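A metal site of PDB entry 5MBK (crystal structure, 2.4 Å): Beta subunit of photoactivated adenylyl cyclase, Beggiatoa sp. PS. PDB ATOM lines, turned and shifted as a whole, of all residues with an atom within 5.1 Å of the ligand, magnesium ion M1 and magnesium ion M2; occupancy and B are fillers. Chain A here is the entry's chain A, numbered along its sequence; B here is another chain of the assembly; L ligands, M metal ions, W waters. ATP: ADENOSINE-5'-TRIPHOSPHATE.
Merely in contact with magnesium ion M1: Arg 287 (3.2 Å).
The nearest printed residue that does not touch magnesium ion M1 is Leu 162 (4.4 Å).
Of the 24 residues printed, 2 come within 4 Å of magnesium ion M2.
Along chain A the residues within 4 Å of magnesium ion M2 span positions 160 to 204.
Magnesium ion M2 is bound by water W2, at 2.0 Å.
Magnesium ion M2 is bound by an oxygen (O2A) of the ligand.
OD1 of Asp 204 binds magnesium ion M2 (2.3 Å).
OD2 of Asp 160 binds magnesium ion M2 (2.4 Å).
Water W1 bridges O2B of the ligand and OG1 of Thr 166.
The guanidinium group (NH2) of Arg 287 lies within hydrogen-bond range of the backbone carbonyl oxygen (O) of Asp 160.
The backbone carbonyl oxygen of Ile 161 sits close to the guanidinium group of Arg 287 (3.0 Å).
The side-chain carboxylate of Asp 274 of chain B is in hydrogen-bond range of the side-chain hydroxyl of Ser 165 (3.1 Å).
O of Leu 271 of chain B sits close to N3 of the ligand, 3.5 Å away.
Residues that only touch the ligand: Leu 162, Ile 202 of chain A, Gly 203, Ile 202 of chain B, Met 207 of chain B, Leu 272 of chain B and Val 276 of chain B.
Hydrophobic or aromatic side chains within 4 Å of the ligand: Leu 162, Phe 164, Ile 202 of chain A, Ile 202 of chain B, Met 207 of chain B, Leu 272 of chain B and Val 276 of chain B.
Of the 24 residues printed, 18 come within 4 Å of the ligand.
O3G of the ligand is bound to magnesium ion M1.
O1B of the ligand is bound to magnesium ion M1 (2.1 Å).
OD1 of Asp 160 binds magnesium ion M1 (2.1 Å).
Magnesium ion M1 is bound by an oxygen (O2A) of the ligand (2.2 Å).
The backbone carbonyl oxygen (O) of Ile 161 binds magnesium ion M1, 2.2 Å away.
OD2 of Asp 204 is bound to magnesium ion M1 (2.2 Å).
O2' of the ligand lies within hydrogen-bond range of O of Gly 273 of chain B, at 2.5 Å.
N of Ser 165 lies within hydrogen-bond range of O2B of the ligand, 2.8 Å away.
The side-chain hydroxyl (OG) of Ser 165 lies within hydrogen-bond range of an oxygen (O2B) of the ligand (2.7 Å).
The backbone NH (N) of Phe 164 lies within hydrogen-bond range of an oxygen (O2B) of the ligand, 3.1 Å away.
The guanidinium group of Arg 287 lies within salt-bridge range of an oxygen (O2G) of the ligand (2.8 Å).
N of Ala 163 is in hydrogen-bond range of O2G of the ligand (2.8 Å).
The backbone NH (N) of Asn 277 of chain B sits at hydrogen-bond distance from an oxygen (O2') of the ligand (2.9 Å).
An oxygen (O3') of the ligand lies within hydrogen-bond range of the backbone NH (N) of Asp 274 of chain B, 3.4 Å away.
The side-chain carboxylate of Asp 274 of chain B sits at hydrogen-bond distance from an oxygen (O3') of the ligand (3.2 Å).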
ATOM      1  N   ASP A 160       3.769 -12.381 -24.366  1.00  0.00           N
ATOM      2  CA  ASP A 160       5.022 -12.100 -23.687  1.00  0.00           C
ATOM      3  C   ASP A 160       5.935 -11.361 -24.647  1.00  0.00           C
ATOM      4  O   ASP A 160       6.039 -11.755 -25.815  1.00  0.00           O
ATOM      5  CB  ASP A 160       5.640 -13.448 -23.275  1.00  0.00           C
ATOM      6  CG  ASP A 160       6.844 -13.295 -22.442  1.00  0.00           C
ATOM      7  OD1 ASP A 160       7.857 -12.847 -22.965  1.00  0.00           O
ATOM      8  OD2 ASP A 160       6.760 -13.682 -21.254  1.00  0.00           O
ATOM      9  N   ILE A 161       6.638 -10.327 -24.151  1.00  0.00           N
ATOM     10  CA  ILE A 161       7.421  -9.460 -25.030  1.00  0.00           C
ATOM     11  C   ILE A 161       8.788 -10.098 -25.318  1.00  0.00           C
ATOM     12  O   ILE A 161       9.477 -10.607 -24.426  1.00  0.00           O
ATOM     13  CB  ILE A 161       7.579  -8.057 -24.409  1.00  0.00           C
ATOM     14  CG1 ILE A 161       6.182  -7.355 -24.268  1.00  0.00           C
ATOM     15  CG2 ILE A 161       8.591  -7.261 -25.229  1.00  0.00           C
ATOM     16  CD1 ILE A 161       6.221  -6.026 -23.369  1.00  0.00           C
ATOM     17  N   LEU A 162       9.178 -10.066 -26.593  1.00  0.00           N
ATOM     18  CA  LEU A 162      10.458 -10.627 -27.025  1.00  0.00           C
ATOM     19  C   LEU A 162      11.582  -9.763 -26.490  1.00  0.00           C
ATOM     20  O   LEU A 162      11.591  -8.542 -26.716  1.00  0.00           O
ATOM     21  CB  LEU A 162      10.507 -10.678 -28.550  1.00  0.00           C
ATOM     22  CG  LEU A 162      11.822 -11.107 -29.194  1.00  0.00           C
ATOM     23  CD1 LEU A 162      11.988 -12.600 -28.984  1.00  0.00           C
ATOM     24  CD2 LEU A 162      11.799 -10.740 -30.692  1.00  0.00           C
ATOM     25  N   ALA A 163      12.503 -10.388 -25.745  1.00  0.00           N
ATOM     26  CA  ALA A 163      13.746  -9.731 -25.296  1.00  0.00           C
ATOM     27  C   ALA A 163      13.438  -8.439 -24.549  1.00  0.00           C
ATOM     28  O   ALA A 163      14.079  -7.407 -24.763  1.00  0.00           O
ATOM     29  CB  ALA A 163      14.687  -9.461 -26.487  1.00  0.00           C
ATOM     30  N   PHE A 164      12.439  -8.473 -23.663  1.00  0.00           N
ATOM     31  CA  PHE A 164      12.112  -7.277 -22.881  1.00  0.00           C
ATOM     32  C   PHE A 164      13.297  -6.769 -22.058  1.00  0.00           C
ATOM     33  O   PHE A 164      13.500  -5.545 -21.946  1.00  0.00           O
ATOM     34  CB  PHE A 164      10.906  -7.570 -21.972  1.00  0.00           C
ATOM     35  CG  PHE A 164      10.441  -6.374 -21.181  1.00  0.00           C
ATOM     36  CD1 PHE A 164       9.498  -5.501 -21.707  1.00  0.00           C
ATOM     37  CD2 PHE A 164      10.945  -6.144 -19.907  1.00  0.00           C
ATOM     38  CE1 PHE A 164       9.077  -4.420 -20.994  1.00  0.00           C
ATOM     39  CE2 PHE A 164      10.540  -5.050 -19.185  1.00  0.00           C
ATOM     40  CZ  PHE A 164       9.604  -4.192 -19.726  1.00  0.00           C
ATOM     41  N   SER A 165      14.115  -7.661 -21.472  1.00  0.00           N
ATOM     42  CA  SER A 165      15.284  -7.207 -20.698  1.00  0.00           C
ATOM     43  C   SER A 165      16.191  -6.338 -21.535  1.00  0.00           C
ATOM     44  O   SER A 165      16.590  -5.243 -21.138  1.00  0.00           O
ATOM     45  CB  SER A 165      16.083  -8.392 -20.185  1.00  0.00           C
ATOM     46  OG  SER A 165      15.225  -9.368 -19.682  1.00  0.00           O
ATOM     47  N   THR A 166      16.572  -6.848 -22.696  1.00  0.00           N
ATOM     48  CA  THR A 166      17.424  -6.145 -23.633  1.00  0.00           C
ATOM     49  C   THR A 166      16.766  -4.869 -24.135  1.00  0.00           C
ATOM     50  O   THR A 166      17.416  -3.816 -24.240  1.00  0.00           O
ATOM     51  CB  THR A 166      17.726  -7.082 -24.797  1.00  0.00           C
ATOM     52  OG1 THR A 166      18.286  -8.303 -24.298  1.00  0.00           O
ATOM     53  CG2 THR A 166      18.638  -6.440 -25.764  1.00  0.00           C
ATOM     54  N   ILE A 202       2.023 -10.633 -15.647  1.00  0.00           N
ATOM     55  CA  ILE A 202       3.205 -11.197 -15.038  1.00  0.00           C
ATOM     56  C   ILE A 202       4.407 -10.605 -15.773  1.00  0.00           C
ATOM     57  O   ILE A 202       4.839 -11.151 -16.789  1.00  0.00           O
ATOM     58  CB  ILE A 202       3.232 -12.728 -15.091  1.00  0.00           C
ATOM     59  CG1 ILE A 202       1.833 -13.297 -14.863  1.00  0.00           C
ATOM     60  CG2 ILE A 202       4.213 -13.274 -14.056  1.00  0.00           C
ATOM     61  CD1 ILE A 202       1.743 -14.794 -14.922  1.00  0.00           C
ATOM     62  N   GLY A 203       4.954  -9.494 -15.264  1.00  0.00           N
ATOM     63  CA  GLY A 203       6.134  -8.915 -15.867  1.00  0.00           C
ATOM     64  C   GLY A 203       5.801  -8.257 -17.186  1.00  0.00           C
ATOM     65  O   GLY A 203       5.047  -7.282 -17.256  1.00  0.00           O
ATOM     66  N   ASP A 204       6.366  -8.790 -18.267  1.00  0.00           N
ATOM     67  CA  ASP A 204       6.090  -8.318 -19.611  1.00  0.00           C
ATOM     68  C   ASP A 204       5.023  -9.178 -20.304  1.00  0.00           C
ATOM     69  O   ASP A 204       5.049  -9.319 -21.533  1.00  0.00           O
ATOM     70  CB  ASP A 204       7.377  -8.325 -20.431  1.00  0.00           C
ATOM     71  CG  ASP A 204       8.000  -9.745 -20.531  1.00  0.00           C
ATOM     72  OD1 ASP A 204       7.858 -10.524 -19.539  1.00  0.00           O
ATOM     73  OD2 ASP A 204       8.635 -10.073 -21.593  1.00  0.00           O
ATOM     74  N   CYS A 205       4.109  -9.767 -19.519  1.00  0.00           N
ATOM     75  CA  CYS A 205       3.330 -10.917 -19.950  1.00  0.00           C
ATOM     76  C   CYS A 205       1.853 -10.811 -19.560  1.00  0.00           C
ATOM     77  O   CYS A 205       1.518 -10.426 -18.436  1.00  0.00           O
ATOM     78  CB  CYS A 205       3.929 -12.208 -19.379  1.00  0.00           C
ATOM     79  SG  CYS A 205       2.845 -13.583 -19.456  1.00  0.00           S
ATOM     80  N   ARG A 287       9.781 -18.273 -29.487  1.00  0.00           N
ATOM     81  CA  ARG A 287      11.110 -17.661 -29.574  1.00  0.00           C
ATOM     82  C   ARG A 287      12.027 -18.398 -30.560  1.00  0.00           C
ATOM     83  O   ARG A 287      12.799 -17.765 -31.281  1.00  0.00           O
ATOM     84  CB  ARG A 287      11.788 -17.616 -28.196  1.00  0.00           C
ATOM     85  CG  ARG A 287      11.896 -16.247 -27.561  1.00  0.00           C
ATOM     86  CD  ARG A 287      10.568 -15.543 -27.630  1.00  0.00           C
ATOM     87  NE  ARG A 287      10.316 -14.657 -26.505  1.00  0.00           N
ATOM     88  CZ  ARG A 287       9.095 -14.249 -26.194  1.00  0.00           C
ATOM     89  NH1 ARG A 287       8.074 -14.652 -26.935  1.00  0.00           N
ATOM     90  NH2 ARG A 287       8.869 -13.448 -25.171  1.00  0.00           N
ATOM     91  N   PHE B 158      10.805 -15.653  -3.916  1.00  0.00           N
ATOM     92  CA  PHE B 158       9.938 -16.567  -4.654  1.00  0.00           C
ATOM     93  C   PHE B 158       9.872 -17.863  -3.862  1.00  0.00           C
ATOM     94  O   PHE B 158      10.910 -18.426  -3.484  1.00  0.00           O
ATOM     95  CB  PHE B 158      10.486 -16.847  -6.066  1.00  0.00           C
ATOM     96  CG  PHE B 158       9.746 -16.138  -7.147  1.00  0.00           C
ATOM     97  CD1 PHE B 158      10.009 -14.820  -7.448  1.00  0.00           C
ATOM     98  CD2 PHE B 158       8.782 -16.792  -7.892  1.00  0.00           C
ATOM     99  CE1 PHE B 158       9.335 -14.163  -8.487  1.00  0.00           C
ATOM    100  CE2 PHE B 158       8.102 -16.158  -8.931  1.00  0.00           C
ATOM    101  CZ  PHE B 158       8.385 -14.841  -9.221  1.00  0.00           C
ATOM    102  N   ILE B 202       1.316 -16.649  -7.881  1.00  0.00           N
ATOM    103  CA  ILE B 202       1.414 -17.183  -9.227  1.00  0.00           C
ATOM    104  C   ILE B 202       1.309 -18.699  -9.104  1.00  0.00           C
ATOM    105  O   ILE B 202       2.318 -19.378  -8.906  1.00  0.00           O
ATOM    106  CB  ILE B 202       2.722 -16.779  -9.921  1.00  0.00           C
ATOM    107  CG1 ILE B 202       3.100 -15.341  -9.570  1.00  0.00           C
ATOM    108  CG2 ILE B 202       2.580 -16.946 -11.432  1.00  0.00           C
ATOM    109  CD1 ILE B 202       4.379 -14.855 -10.186  1.00  0.00           C
ATOM    110  N   MET B 207       5.207 -14.555  -4.439  1.00  0.00           N
ATOM    111  CA  MET B 207       6.222 -13.592  -4.774  1.00  0.00           C
ATOM    112  C   MET B 207       6.178 -12.471  -3.759  1.00  0.00           C
ATOM    113  O   MET B 207       5.109 -11.980  -3.404  1.00  0.00           O
ATOM    114  CB  MET B 207       6.050 -13.050  -6.191  1.00  0.00           C
ATOM    115  CG  MET B 207       7.006 -11.886  -6.503  1.00  0.00           C
ATOM    116  SD  MET B 207       6.994 -11.360  -8.244  1.00  0.00           S
ATOM    117  CE  MET B 207       5.568 -10.323  -8.329  1.00  0.00           C
ATOM    118  N   THR B 270       3.091  -3.369  -9.078  1.00  0.00           N
ATOM    119  CA  THR B 270       3.988  -4.524  -9.042  1.00  0.00           C
ATOM    120  C   THR B 270       5.438  -4.081  -9.216  1.00  0.00           C
ATOM    121  O   THR B 270       5.766  -2.901  -9.197  1.00  0.00           O
ATOM    122  CB  THR B 270       3.588  -5.523 -10.139  1.00  0.00           C
ATOM    123  OG1 THR B 270       4.329  -6.749  -9.971  1.00  0.00           O
ATOM    124  CG2 THR B 270       3.930  -4.960 -11.489  1.00  0.00           C
ATOM    125  N   LEU B 271       6.310  -5.075  -9.391  1.00  0.00           N
ATOM    126  CA  LEU B 271       7.742  -4.891  -9.462  1.00  0.00           C
ATOM    127  C   LEU B 271       8.202  -5.542 -10.751  1.00  0.00           C
ATOM    128  O   LEU B 271       7.743  -6.622 -11.074  1.00  0.00           O
ATOM    129  CB  LEU B 271       8.474  -5.489  -8.234  1.00  0.00           C
ATOM    130  CG  LEU B 271       8.017  -5.118  -6.822  1.00  0.00           C
ATOM    131  CD1 LEU B 271       8.575  -6.071  -5.773  1.00  0.00           C
ATOM    132  CD2 LEU B 271       8.529  -3.726  -6.544  1.00  0.00           C
ATOM    133  N   LEU B 272       9.053  -4.832 -11.498  1.00  0.00           N
ATOM    134  CA  LEU B 272       9.577  -5.267 -12.795  1.00  0.00           C
ATOM    135  C   LEU B 272      11.090  -5.095 -12.780  1.00  0.00           C
ATOM    136  O   LEU B 272      11.596  -4.036 -12.368  1.00  0.00           O
ATOM    137  CB  LEU B 272       8.924  -4.462 -13.944  1.00  0.00           C
ATOM    138  CG  LEU B 272       9.182  -4.790 -15.417  1.00  0.00           C
ATOM    139  CD1 LEU B 272       8.650  -6.176 -15.789  1.00  0.00           C
ATOM    140  CD2 LEU B 272       8.559  -3.751 -16.331  1.00  0.00           C
ATOM    141  N   GLY B 273      11.805  -6.115 -13.194  1.00  0.00           N
ATOM    142  CA  GLY B 273      13.252  -6.047 -13.290  1.00  0.00           C
ATOM    143  C   GLY B 273      13.765  -7.461 -13.393  1.00  0.00           C
ATOM    144  O   GLY B 273      13.030  -8.410 -13.141  1.00  0.00           O
ATOM    145  N   ASP B 274      15.052  -7.573 -13.781  1.00  0.00           N
ATOM    146  CA  ASP B 274      15.689  -8.904 -13.965  1.00  0.00           C
ATOM    147  C   ASP B 274      15.867  -9.670 -12.653  1.00  0.00           C
ATOM    148  O   ASP B 274      15.811 -10.894 -12.658  1.00  0.00           O
ATOM    149  CB  ASP B 274      17.077  -8.756 -14.639  1.00  0.00           C
ATOM    150  CG  ASP B 274      16.982  -8.288 -16.112  1.00  0.00           C
ATOM    151  OD1 ASP B 274      15.967  -8.587 -16.797  1.00  0.00           O
ATOM    152  OD2 ASP B 274      17.930  -7.601 -16.579  1.00  0.00           O
ATOM    153  N   ALA B 275      16.165  -8.991 -11.534  1.00  0.00           N
ATOM    154  CA  ALA B 275      16.128  -9.669 -10.231  1.00  0.00           C
ATOM    155  C   ALA B 275      14.908 -10.561 -10.086  1.00  0.00           C
ATOM    156  O   ALA B 275      14.998 -11.626  -9.440  1.00  0.00           O
ATOM    157  CB  ALA B 275      16.149  -8.683  -9.075  1.00  0.00           C
ATOM    158  N   VAL B 276      13.756 -10.170 -10.661  1.00  0.00           N
ATOM    159  CA  VAL B 276      12.577 -11.006 -10.503  1.00  0.00           C
ATOM    160  C   VAL B 276      12.845 -12.373 -11.107  1.00  0.00           C
ATOM    161  O   VAL B 276      12.691 -13.423 -10.460  1.00  0.00           O
ATOM    162  CB  VAL B 276      11.338 -10.331 -11.101  1.00  0.00           C
ATOM    163  CG1 VAL B 276      10.110 -11.242 -10.969  1.00  0.00           C
ATOM    164  CG2 VAL B 276      11.121  -8.999 -10.406  1.00  0.00           C
ATOM    165  N   ASN B 277      13.315 -12.374 -12.343  1.00  0.00           N
ATOM    166  CA  ASN B 277      13.586 -13.603 -13.025  1.00  0.00           C
ATOM    167  C   ASN B 277      14.607 -14.459 -12.285  1.00  0.00           C
ATOM    168  O   ASN B 277      14.482 -15.683 -12.259  1.00  0.00           O
ATOM    169  CB  ASN B 277      14.096 -13.293 -14.404  1.00  0.00           C
ATOM    170  CG  ASN B 277      14.145 -14.501 -15.229  1.00  0.00           C
ATOM    171  OD1 ASN B 277      13.112 -14.925 -15.734  1.00  0.00           O
ATOM    172  ND2 ASN B 277      15.323 -15.111 -15.338  1.00  0.00           N
ATOM    173  N   ARG B 281      14.339 -18.379 -10.766  1.00  0.00           N
ATOM    174  CA  ARG B 281      15.205 -19.500 -11.138  1.00  0.00           C
ATOM    175  C   ARG B 281      15.967 -20.081  -9.957  1.00  0.00           C
ATOM    176  O   ARG B 281      16.227 -21.292  -9.953  1.00  0.00           O
ATOM    177  CB  ARG B 281      16.241 -19.116 -12.205  1.00  0.00           C
ATOM    178  CG  ARG B 281      15.661 -18.397 -13.373  1.00  0.00           C
ATOM    179  CD  ARG B 281      14.984 -19.352 -14.343  1.00  0.00           C
ATOM    180  NE  ARG B 281      14.688 -18.717 -15.617  1.00  0.00           N
ATOM    181  CZ  ARG B 281      13.706 -17.821 -15.791  1.00  0.00           C
ATOM    182  NH1 ARG B 281      13.492 -17.287 -16.992  1.00  0.00           N
ATOM    183  NH2 ARG B 281      12.914 -17.445 -14.775  1.00  0.00           N
HETATM  184  PG  ATP L   1      12.206 -13.521 -23.791  1.00  0.00           P
HETATM  185  O1G ATP L   1      12.583 -14.944 -23.391  1.00  0.00           O
HETATM  186  O2G ATP L   1      12.332 -13.163 -25.265  1.00  0.00           O
HETATM  187  O3G ATP L   1      10.862 -13.119 -23.236  1.00  0.00           O
HETATM  188  PB  ATP L   1      12.855 -11.409 -21.983  1.00  0.00           P
HETATM  189  O1B ATP L   1      11.554 -10.805 -22.408  1.00  0.00           O
HETATM  190  O2B ATP L   1      13.973 -10.427 -21.812  1.00  0.00           O
HETATM  191  O3B ATP L   1      13.285 -12.590 -23.009  1.00  0.00           O
HETATM  192  PA  ATP L   1      11.393 -12.598 -19.753  1.00  0.00           P
HETATM  193  O1A ATP L   1      11.575 -13.957 -19.112  1.00  0.00           O
HETATM  194  O2A ATP L   1      10.166 -12.354 -20.594  1.00  0.00           O
HETATM  195  O3A ATP L   1      12.723 -12.245 -20.611  1.00  0.00           O
HETATM  196  O5' ATP L   1      11.484 -11.449 -18.618  1.00  0.00           O
HETATM  197  C5' ATP L   1      11.123 -10.092 -18.845  1.00  0.00           C
HETATM  198  C4' ATP L   1      11.083  -9.312 -17.538  1.00  0.00           C
HETATM  199  O4' ATP L   1       9.922  -9.690 -16.775  1.00  0.00           O
HETATM  200  C3' ATP L   1      12.314  -9.582 -16.677  1.00  0.00           C
HETATM  201  O3' ATP L   1      12.843  -8.327 -16.215  1.00  0.00           O
HETATM  202  C2' ATP L   1      11.761 -10.481 -15.575  1.00  0.00           C
HETATM  203  O2' ATP L   1      12.435 -10.488 -14.326  1.00  0.00           O
HETATM  204  C1' ATP L   1      10.375  -9.916 -15.436  1.00  0.00           C
HETATM  205  N9  ATP L   1       9.515 -10.867 -14.721  1.00  0.00           N
HETATM  206  C8  ATP L   1       9.453 -12.198 -14.876  1.00  0.00           C
HETATM  207  N7  ATP L   1       8.524 -12.729 -14.056  1.00  0.00           N
HETATM  208  C5  ATP L   1       7.968 -11.702 -13.373  1.00  0.00           C
HETATM  209  C6  ATP L   1       6.947 -11.538 -12.318  1.00  0.00           C
HETATM  210  N6  ATP L   1       6.297 -12.629 -11.830  1.00  0.00           N
HETATM  211  N1  ATP L   1       6.686 -10.276 -11.874  1.00  0.00           N
HETATM  212  C2  ATP L   1       7.332  -9.184 -12.345  1.00  0.00           C
HETATM  213  N3  ATP L   1       8.296  -9.255 -13.287  1.00  0.00           N
HETATM  214  C4  ATP L   1       8.637 -10.469 -13.816  1.00  0.00           C
HETATM  215 MG    MG M   1       9.662 -11.755 -22.605  1.00  0.00          MG
HETATM  216 MG    MG M   2       8.188 -12.776 -19.590  1.00  0.00          MG
HETATM  217  O   HOH W   1      16.230 -10.395 -23.277  1.00  0.00           O
HETATM  218  O   HOH W   2       8.436 -14.716 -19.801  1.00  0.00           O
